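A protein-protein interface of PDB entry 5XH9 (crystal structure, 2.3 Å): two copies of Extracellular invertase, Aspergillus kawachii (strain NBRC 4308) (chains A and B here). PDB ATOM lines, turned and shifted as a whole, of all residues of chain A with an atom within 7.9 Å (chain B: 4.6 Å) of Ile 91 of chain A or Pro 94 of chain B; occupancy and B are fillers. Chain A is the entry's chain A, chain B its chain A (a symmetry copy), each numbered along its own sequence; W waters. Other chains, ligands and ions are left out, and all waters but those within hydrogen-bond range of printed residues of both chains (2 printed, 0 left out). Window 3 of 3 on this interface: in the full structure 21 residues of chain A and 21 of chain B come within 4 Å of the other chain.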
ATOM      1  N   PRO A  88     -31.818  17.821  26.069  1.00  0.00           N
ATOM      2  CA  PRO A  88     -31.185  17.526  24.783  1.00  0.00           C
ATOM      3  C   PRO A  88     -32.192  17.495  23.632  1.00  0.00           C
ATOM      4  O   PRO A  88     -33.383  17.561  23.868  1.00  0.00           O
ATOM      5  CB  PRO A  88     -30.611  16.120  24.988  1.00  0.00           C
ATOM      6  CG  PRO A  88     -31.489  15.504  26.026  1.00  0.00           C
ATOM      7  CD  PRO A  88     -31.780  16.656  26.964  1.00  0.00           C
ATOM      8  N   GLY A  89     -31.702  17.401  22.402  1.00  0.00           N
ATOM      9  CA  GLY A  89     -32.569  17.284  21.201  1.00  0.00           C
ATOM     10  C   GLY A  89     -32.629  18.530  20.316  1.00  0.00           C
ATOM     11  O   GLY A  89     -33.440  18.594  19.373  1.00  0.00           O
ATOM     12  N   GLY A  90     -31.782  19.522  20.621  1.00  0.00           N
ATOM     13  CA  GLY A  90     -31.616  20.687  19.756  1.00  0.00           C
ATOM     14  C   GLY A  90     -30.526  20.447  18.741  1.00  0.00           C
ATOM     15  O   GLY A  90     -29.887  19.393  18.714  1.00  0.00           O
ATOM     16  N   ILE A  91     -30.290  21.462  17.927  1.00  0.00           N
ATOM     17  CA  ILE A  91     -29.338  21.379  16.850  1.00  0.00           C
ATOM     18  C   ILE A  91     -27.892  21.158  17.355  1.00  0.00           C
ATOM     19  O   ILE A  91     -27.137  20.351  16.777  1.00  0.00           O
ATOM     20  CB  ILE A  91     -29.425  22.651  15.989  1.00  0.00           C
ATOM     21  CG1 ILE A  91     -30.806  22.715  15.295  1.00  0.00           C
ATOM     22  CG2 ILE A  91     -28.263  22.731  14.997  1.00  0.00           C
ATOM     23  CD1 ILE A  91     -31.108  21.573  14.344  1.00  0.00           C
ATOM     24  N   ASN A  92     -27.521  21.890  18.411  1.00  0.00           N
ATOM     25  CA  ASN A  92     -26.182  21.815  19.003  1.00  0.00           C
ATOM     26  C   ASN A  92     -25.990  20.640  19.946  1.00  0.00           C
ATOM     27  O   ASN A  92     -24.857  20.151  20.070  1.00  0.00           O
ATOM     28  CB  ASN A  92     -25.845  23.103  19.763  1.00  0.00           C
ATOM     29  CG  ASN A  92     -25.917  24.346  18.886  1.00  0.00           C
ATOM     30  OD1 ASN A  92     -26.005  24.261  17.647  1.00  0.00           O
ATOM     31  ND2 ASN A  92     -25.886  25.519  19.531  1.00  0.00           N
ATOM     32  N   ASP A  93     -27.076  20.183  20.576  1.00  0.00           N
ATOM     33  CA  ASP A  93     -27.053  19.129  21.609  1.00  0.00           C
ATOM     34  C   ASP A  93     -28.070  18.012  21.303  1.00  0.00           C
ATOM     35  O   ASP A  93     -28.919  17.673  22.146  1.00  0.00           O
ATOM     36  CB  ASP A  93     -27.328  19.733  23.012  1.00  0.00           C
ATOM     37  CG  ASP A  93     -28.574  20.634  23.059  1.00  0.00           C
ATOM     38  OD1 ASP A  93     -29.372  20.608  22.103  1.00  0.00           O
ATOM     39  OD2 ASP A  93     -28.753  21.377  24.049  1.00  0.00           O
ATOM     40  N   PRO A  94     -27.975  17.400  20.108  1.00  0.00           N
ATOM     41  CA  PRO A  94     -29.004  16.443  19.721  1.00  0.00           C
ATOM     42  C   PRO A  94     -29.002  15.172  20.558  1.00  0.00           C
ATOM     43  O   PRO A  94     -30.027  14.504  20.612  1.00  0.00           O
ATOM     44  CB  PRO A  94     -28.665  16.122  18.264  1.00  0.00           C
ATOM     45  CG  PRO A  94     -27.178  16.316  18.203  1.00  0.00           C
ATOM     46  CD  PRO A  94     -26.894  17.465  19.117  1.00  0.00           C
ATOM     47  N   VAL A  95     -27.876  14.864  21.207  1.00  0.00           N
ATOM     48  CA  VAL A  95     -27.734  13.637  21.987  1.00  0.00           C
ATOM     49  C   VAL A  95     -27.749  13.874  23.485  1.00  0.00           C
ATOM     50  O   VAL A  95     -28.377  13.123  24.198  1.00  0.00           O
ATOM     51  CB  VAL A  95     -26.499  12.830  21.509  1.00  0.00           C
ATOM     52  CG1 VAL A  95     -26.286  11.604  22.362  1.00  0.00           C
ATOM     53  CG2 VAL A  95     -26.732  12.357  20.070  1.00  0.00           C
ATOM     54  N   TYR A 115     -22.929  25.826  28.627  1.00  0.00           N
ATOM     55  CA  TYR A 115     -23.021  24.383  28.960  1.00  0.00           C
ATOM     56  C   TYR A 115     -22.483  23.500  27.874  1.00  0.00           C
ATOM     57  O   TYR A 115     -22.356  23.915  26.715  1.00  0.00           O
ATOM     58  CB  TYR A 115     -24.465  23.984  29.216  1.00  0.00           C
ATOM     59  CG  TYR A 115     -25.351  23.897  27.975  1.00  0.00           C
ATOM     60  CD1 TYR A 115     -25.933  25.054  27.417  1.00  0.00           C
ATOM     61  CD2 TYR A 115     -25.644  22.659  27.386  1.00  0.00           C
ATOM     62  CE1 TYR A 115     -26.759  24.969  26.300  1.00  0.00           C
ATOM     63  CE2 TYR A 115     -26.467  22.564  26.265  1.00  0.00           C
ATOM     64  CZ  TYR A 115     -27.027  23.703  25.726  1.00  0.00           C
ATOM     65  OH  TYR A 115     -27.846  23.605  24.603  1.00  0.00           O
ATOM     66  N   SER A 117     -22.938  20.978  25.206  1.00  0.00           N
ATOM     67  CA  SER A 117     -23.870  20.403  24.239  1.00  0.00           C
ATOM     68  C   SER A 117     -23.206  19.204  23.543  1.00  0.00           C
ATOM     69  O   SER A 117     -22.097  19.344  23.005  1.00  0.00           O
ATOM     70  CB  SER A 117     -24.250  21.479  23.210  1.00  0.00           C
ATOM     71  OG  SER A 117     -23.182  22.354  22.877  1.00  0.00           O
ATOM     72  N   VAL A 118     -23.881  18.053  23.532  1.00  0.00           N
ATOM     73  CA  VAL A 118     -23.293  16.774  23.093  1.00  0.00           C
ATOM     74  C   VAL A 118     -23.982  16.245  21.834  1.00  0.00           C
ATOM     75  O   VAL A 118     -25.218  16.231  21.764  1.00  0.00           O
ATOM     76  CB  VAL A 118     -23.381  15.718  24.209  1.00  0.00           C
ATOM     77  CG1 VAL A 118     -22.786  14.384  23.785  1.00  0.00           C
ATOM     78  CG2 VAL A 118     -22.679  16.219  25.447  1.00  0.00           C
ATOM     79  N   SER A 119     -23.173  15.882  20.832  1.00  0.00           N
ATOM     80  CA  SER A 119     -23.642  15.423  19.511  1.00  0.00           C
ATOM     81  C   SER A 119     -23.257  13.983  19.158  1.00  0.00           C
ATOM     82  O   SER A 119     -23.833  13.392  18.240  1.00  0.00           O
ATOM     83  CB  SER A 119     -23.098  16.361  18.422  1.00  0.00           C
ATOM     84  OG  SER A 119     -23.527  17.713  18.624  1.00  0.00           O
ATOM     85  N   THR A 135     -19.205  20.381  22.703  1.00  0.00           N
ATOM     86  CA  THR A 135     -19.045  21.782  22.369  1.00  0.00           C
ATOM     87  C   THR A 135     -19.657  22.562  23.505  1.00  0.00           C
ATOM     88  O   THR A 135     -20.357  21.992  24.339  1.00  0.00           O
ATOM     89  CB  THR A 135     -19.773  22.148  21.064  1.00  0.00           C
ATOM     90  OG1 THR A 135     -21.168  21.882  21.203  1.00  0.00           O
ATOM     91  CG2 THR A 135     -19.223  21.347  19.873  1.00  0.00           C
ATOM     92  N   SER A 137     -22.208  25.708  24.397  1.00  0.00           N
ATOM     93  CA  SER A 137     -23.314  26.460  23.820  1.00  0.00           C
ATOM     94  C   SER A 137     -23.971  27.362  24.860  1.00  0.00           C
ATOM     95  O   SER A 137     -23.827  27.145  26.081  1.00  0.00           O
ATOM     96  CB  SER A 137     -24.367  25.498  23.227  1.00  0.00           C
ATOM     97  OG  SER A 137     -23.892  24.876  22.034  1.00  0.00           O
ATOM     98  N   LYS A 150     -32.325  28.038  24.355  1.00  0.00           N
ATOM     99  CA  LYS A 150     -31.075  27.968  23.616  1.00  0.00           C
ATOM    100  C   LYS A 150     -30.987  29.078  22.569  1.00  0.00           C
ATOM    101  O   LYS A 150     -31.919  29.287  21.825  1.00  0.00           O
ATOM    102  CB  LYS A 150     -30.972  26.626  22.894  1.00  0.00           C
ATOM    103  CG  LYS A 150     -30.830  25.418  23.809  1.00  0.00           C
ATOM    104  CD  LYS A 150     -31.237  24.142  23.101  1.00  0.00           C
ATOM    105  CE  LYS A 150     -31.544  23.035  24.082  1.00  0.00           C
ATOM    106  NZ  LYS A 150     -31.658  21.692  23.441  1.00  0.00           N
ATOM    107  N   LEU A 151     -29.867  29.776  22.499  1.00  0.00           N
ATOM    108  CA  LEU A 151     -29.644  30.689  21.375  1.00  0.00           C
ATOM    109  C   LEU A 151     -29.699  29.888  20.091  1.00  0.00           C
ATOM    110  O   LEU A 151     -29.143  28.759  20.012  1.00  0.00           O
ATOM    111  CB  LEU A 151     -28.286  31.401  21.456  1.00  0.00           C
ATOM    112  CG  LEU A 151     -28.055  32.352  22.636  1.00  0.00           C
ATOM    113  CD1 LEU A 151     -26.851  33.229  22.335  1.00  0.00           C
ATOM    114  CD2 LEU A 151     -29.293  33.208  22.941  1.00  0.00           C
ATOM    115  N   ASP A 152     -30.365  30.478  19.100  1.00  0.00           N
ATOM    116  CA  ASP A 152     -30.588  29.846  17.812  1.00  0.00           C
ATOM    117  C   ASP A 152     -29.332  30.106  16.951  1.00  0.00           C
ATOM    118  O   ASP A 152     -29.350  30.794  15.938  1.00  0.00           O
ATOM    119  CB  ASP A 152     -31.890  30.399  17.188  1.00  0.00           C
ATOM    120  CG  ASP A 152     -32.299  29.671  15.934  1.00  0.00           C
ATOM    121  OD1 ASP A 152     -31.988  28.477  15.827  1.00  0.00           O
ATOM    122  OD2 ASP A 152     -32.924  30.284  15.035  1.00  0.00           O
ATOM    123  N   GLN A 153     -28.227  29.533  17.392  1.00  0.00           N
ATOM    124  CA  GLN A 153     -26.957  29.585  16.697  1.00  0.00           C
ATOM    125  C   GLN A 153     -26.128  28.398  17.158  1.00  0.00           C
ATOM    126  O   GLN A 153     -26.522  27.678  18.067  1.00  0.00           O
ATOM    127  CB  GLN A 153     -26.224  30.883  17.024  1.00  0.00           C
ATOM    128  CG  GLN A 153     -25.911  31.026  18.507  1.00  0.00           C
ATOM    129  CD  GLN A 153     -24.821  32.030  18.759  1.00  0.00           C
ATOM    130  OE1 GLN A 153     -25.031  33.211  18.604  1.00  0.00           O
ATOM    131  NE2 GLN A 153     -23.644  31.554  19.107  1.00  0.00           N
ATOM    132  N   GLY A 154     -24.980  28.204  16.526  1.00  0.00           N
ATOM    133  CA  GLY A 154     -24.067  27.153  16.889  1.00  0.00           C
ATOM    134  C   GLY A 154     -23.346  27.429  18.192  1.00  0.00           C
ATOM    135  O   GLY A 154     -23.524  28.483  18.804  1.00  0.00           O
ATOM    136  N   PRO A 155     -22.513  26.477  18.620  1.00  0.00           N
ATOM    137  CA  PRO A 155     -21.805  26.633  19.894  1.00  0.00           C
ATOM    138  C   PRO A 155     -20.844  27.810  19.872  1.00  0.00           C
ATOM    139  O   PRO A 155     -20.343  28.156  18.813  1.00  0.00           O
ATOM    140  CB  PRO A 155     -21.020  25.328  20.026  1.00  0.00           C
ATOM    141  CG  PRO A 155     -20.853  24.872  18.627  1.00  0.00           C
ATOM    142  CD  PRO A 155     -22.109  25.254  17.915  1.00  0.00           C
ATOM    143  N   GLY B  89     -29.844  16.351   6.803  1.00  0.00           N
ATOM    144  CA  GLY B  89     -30.595  15.637   7.867  1.00  0.00           C
ATOM    145  C   GLY B  89     -29.741  14.799   8.819  1.00  0.00           C
ATOM    146  O   GLY B  89     -30.280  14.042   9.648  1.00  0.00           O
ATOM    147  N   GLY B  90     -28.413  14.924   8.697  1.00  0.00           N
ATOM    148  CA  GLY B  90     -27.491  14.318   9.655  1.00  0.00           C
ATOM    149  C   GLY B  90     -27.194  15.270  10.787  1.00  0.00           C
ATOM    150  O   GLY B  90     -27.683  16.400  10.826  1.00  0.00           O
ATOM    151  N   ILE B  91     -26.348  14.811  11.693  1.00  0.00           N
ATOM    152  CA  ILE B  91     -26.011  15.555  12.878  1.00  0.00           C
ATOM    153  C   ILE B  91     -25.293  16.888  12.556  1.00  0.00           C
ATOM    154  O   ILE B  91     -25.589  17.931  13.173  1.00  0.00           O
ATOM    155  CB  ILE B  91     -25.148  14.682  13.805  1.00  0.00           C
ATOM    156  CG1 ILE B  91     -25.981  13.482  14.312  1.00  0.00           C
ATOM    157  CG2 ILE B  91     -24.549  15.507  14.947  1.00  0.00           C
ATOM    158  CD1 ILE B  91     -27.203  13.840  15.134  1.00  0.00           C
ATOM    159  N   ASN B  92     -24.348  16.832  11.612  1.00  0.00           N
ATOM    160  CA  ASN B  92     -23.562  17.998  11.199  1.00  0.00           C
ATOM    161  C   ASN B  92     -24.276  18.905  10.213  1.00  0.00           C
ATOM    162  O   ASN B  92     -24.005  20.115  10.207  1.00  0.00           O
ATOM    163  CB  ASN B  92     -22.227  17.569  10.581  1.00  0.00           C
ATOM    164  CG  ASN B  92     -21.380  16.724  11.524  1.00  0.00           C
ATOM    165  OD1 ASN B  92     -21.664  16.617  12.731  1.00  0.00           O
ATOM    166  ND2 ASN B  92     -20.329  16.107  10.970  1.00  0.00           N
ATOM    167  N   ASP B  93     -25.185  18.338   9.413  1.00  0.00           N
ATOM    168  CA  ASP B  93     -25.886  19.043   8.324  1.00  0.00           C
ATOM    169  C   ASP B  93     -27.413  18.854   8.414  1.00  0.00           C
ATOM    170  O   ASP B  93     -28.062  18.424   7.445  1.00  0.00           O
ATOM    171  CB  ASP B  93     -25.369  18.564   6.941  1.00  0.00           C
ATOM    172  CG  ASP B  93     -25.349  17.033   6.790  1.00  0.00           C
ATOM    173  OD1 ASP B  93     -25.955  16.338   7.627  1.00  0.00           O
ATOM    174  OD2 ASP B  93     -24.720  16.522   5.838  1.00  0.00           O
ATOM    175  N   PRO B  94     -28.012  19.208   9.567  1.00  0.00           N
ATOM    176  CA  PRO B  94     -29.427  18.909   9.747  1.00  0.00           C
ATOM    177  C   PRO B  94     -30.342  19.712   8.833  1.00  0.00           C
ATOM    178  O   PRO B  94     -31.463  19.277   8.597  1.00  0.00           O
ATOM    179  CB  PRO B  94     -29.686  19.271  11.211  1.00  0.00           C
ATOM    180  CG  PRO B  94     -28.684  20.355  11.483  1.00  0.00           C
ATOM    181  CD  PRO B  94     -27.471  19.975  10.695  1.00  0.00           C
ATOM    182  N   VAL B  95     -29.858  20.846   8.320  1.00  0.00           N
ATOM    183  CA  VAL B  95     -30.665  21.732   7.483  1.00  0.00           C
ATOM    184  C   VAL B  95     -30.283  21.683   6.017  1.00  0.00           C
ATOM    185  O   VAL B  95     -31.154  21.664   5.177  1.00  0.00           O
ATOM    186  CB  VAL B  95     -30.673  23.169   8.066  1.00  0.00           C
ATOM    187  CG1 VAL B  95     -31.428  24.116   7.167  1.00  0.00           C
ATOM    188  CG2 VAL B  95     -31.380  23.159   9.425  1.00  0.00           C
ATOM    189  N   ALA B  96     -29.002  21.670   5.670  1.00  0.00           N
ATOM    190  CA  ALA B  96     -28.665  21.669   4.253  1.00  0.00           C
ATOM    191  C   ALA B  96     -27.285  21.125   3.961  1.00  0.00           C
ATOM    192  O   ALA B  96     -26.437  21.013   4.855  1.00  0.00           O
ATOM    193  CB  ALA B  96     -28.839  23.061   3.645  1.00  0.00           C
ATOM    194  N   VAL B 118     -24.680  22.368   6.770  1.00  0.00           N
ATOM    195  CA  VAL B 118     -25.434  23.562   7.195  1.00  0.00           C
ATOM    196  C   VAL B 118     -26.425  23.227   8.312  1.00  0.00           C
ATOM    197  O   VAL B 118     -27.154  22.232   8.216  1.00  0.00           O
ATOM    198  CB  VAL B 118     -26.190  24.184   6.009  1.00  0.00           C
ATOM    199  CG1 VAL B 118     -26.984  25.416   6.415  1.00  0.00           C
ATOM    200  CG2 VAL B 118     -25.218  24.543   4.911  1.00  0.00           C
ATOM    201  N   SER B 119     -26.388  24.025   9.386  1.00  0.00           N
ATOM    202  CA  SER B 119     -27.203  23.825  10.599  1.00  0.00           C
ATOM    203  C   SER B 119     -28.193  24.954  10.900  1.00  0.00           C
ATOM    204  O   SER B 119     -29.124  24.772  11.691  1.00  0.00           O
ATOM    205  CB  SER B 119     -26.278  23.641  11.812  1.00  0.00           C
ATOM    206  OG  SER B 119     -25.404  22.518  11.647  1.00  0.00           O
ATOM    207  N   TYR B 120     -27.997  26.109  10.276  1.00  0.00           N
ATOM    208  CA  TYR B 120     -28.813  27.300  10.520  1.00  0.00           C
ATOM    209  C   TYR B 120     -28.982  28.104   9.232  1.00  0.00           C
ATOM    210  O   TYR B 120     -28.006  28.383   8.539  1.00  0.00           O
ATOM    211  CB  TYR B 120     -28.166  28.194  11.579  1.00  0.00           C
ATOM    212  CG  TYR B 120     -28.074  27.517  12.927  1.00  0.00           C
ATOM    213  CD1 TYR B 120     -29.177  27.471  13.775  1.00  0.00           C
ATOM    214  CD2 TYR B 120     -26.892  26.905  13.356  1.00  0.00           C
ATOM    215  CE1 TYR B 120     -29.104  26.836  15.004  1.00  0.00           C
ATOM    216  CE2 TYR B 120     -26.826  26.270  14.590  1.00  0.00           C
ATOM    217  CZ  TYR B 120     -27.947  26.240  15.394  1.00  0.00           C
ATOM    218  OH  TYR B 120     -27.909  25.629  16.599  1.00  0.00           O
HETATM  219  O   HOH W   1     -27.730  18.441  14.863  1.00  0.00           O
HETATM  220  O   HOH W   2     -29.518  26.280  18.673  1.00  0.00           O
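The side-chain hydroxyl (OG) of Ser 119 of chain A sits at hydrogen-bond distance from the backbone carbonyl oxygen (O) of Asn 92 of chain A (3.1 Å). The side-chain amide nitrogen (ND2) of Asn 92 of chain A is in hydrogen-bond range of the side-chain hydroxyl (OG) of Ser 137 of chain A (3.3 Å). The side-chain amide nitrogen (ND2) of Asn 92 of chain A is in hydrogen-bond range of the backbone carbonyl oxygen (O) of Gln 153 of chain A (2.7 Å). The side-chain hydroxyl (OG) of Ser 119 of chain B lies within hydrogen-bond range of the backbone carbonyl oxygen (O) of Asn 92 of chain B.
Among the printed residues, pairs that only touch across the chains: Gly 154 of chain A with Tyr 120 of chain B, Ile 91 of chain A with Tyr 120 of chain B, Asp 152 of chain A with Tyr 120 of chain B, Ser 119 of chain A with Ile 91 of chain B, Ile 91 of chain A with Ser 119 of chain B, Ile 91 of chain A with Pro 94 of chain B and Pro 94 of chain A with Ile 91 of chain B.
Of chain B, only Pro 94 (3.9 Å), Ser 119 (3.9 Å) and Tyr 120 (3.3 Å) come within 4 Å of Ile 91 of chain A. Pro 94 of chain B touches just one residue of chain A: Ile 91. Of the printed residues of chain B, Pro 94 of chain A touches Ile 91 (3.9 Å). Of the printed residues of chain A, Ser 119 of chain B touches Ile 91. Printed residues of chain B within 4 Å of Gln 153 of chain A: Tyr 120. Lys 150 of chain A touches none of the printed residues of chain B. Gly 89 of chain B touches none of the printed residues of chain A. The nearest printed residue of chain B that does not touch Ile 91 of chain A is Ile 91 of chain B (4.6 Å). The nearest residue of chain A that does not touch Pro 94 of chain B is Asn 92 of chain A (7.2 Å).
Ile 91 of chain A touches Pro 94 of chain B, and with the chains exchanged Pro 94 of chain A touches Ile 91 of chain B. Ile 91 of chain A touches Ser 119 of chain B, and with the chains exchanged Ser 119 of chain A touches Ile 91 of chain B. Positions printed for both chains: 89, 90, 91, 92, 93, 94, 95, 118 and 119. Of the 9 pairs that touch across the chains among the printed residues, 4 have their exchanged pair printed and touching as well.
The side-chain hydroxyl (OH) of Tyr 120 of chain B sits at hydrogen-bond distance from the side-chain amide oxygen (OD1) of Asn 92 of chain A (2.6 Å). The backbone carbonyl oxygen (O) of Gln 153 of chain A lies within hydrogen-bond range of the side-chain hydroxyl (OH) of Tyr 120 of chain B, at 2.9 Å.
Water W2 lies within hydrogen-bond range of OH of Tyr 120 of chain B (2.7 Å), O of Leu 151 of chain A (2.8 Å) and O of Gln 153 of chain A (3.4 Å). Water W1 lies within hydrogen-bond range of the backbone carbonyl oxygen (O) of Ile 91 of chain A and the backbone carbonyl oxygen (O) of Ile 91 of chain B.
Printed residues of chain A that touch a printed residue of chain B: Ile 91, Asn 92, Pro 94, Ser 119, Asp 152, Gln 153 and Gly 154. Hydrophobic or aromatic side chains of chain A that line the printed part of chain B: Ile 91 and Pro 94. Of the 11 printed residues of chain B, 4 touch a printed residue of chain A. Printed residues of chain B that touch a printed residue of chain A: Ile 91, Pro 94, Ser 119 and Tyr 120. Hydrophobic or aromatic side chains of chain B that line the printed part of chain A: Ile 91, Pro 94 and Tyr 120. Along chain B the printed residues that touch a printed residue of chain A span positions 91 to 120. Among the printed residues, 9 pairs touch across the chains.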
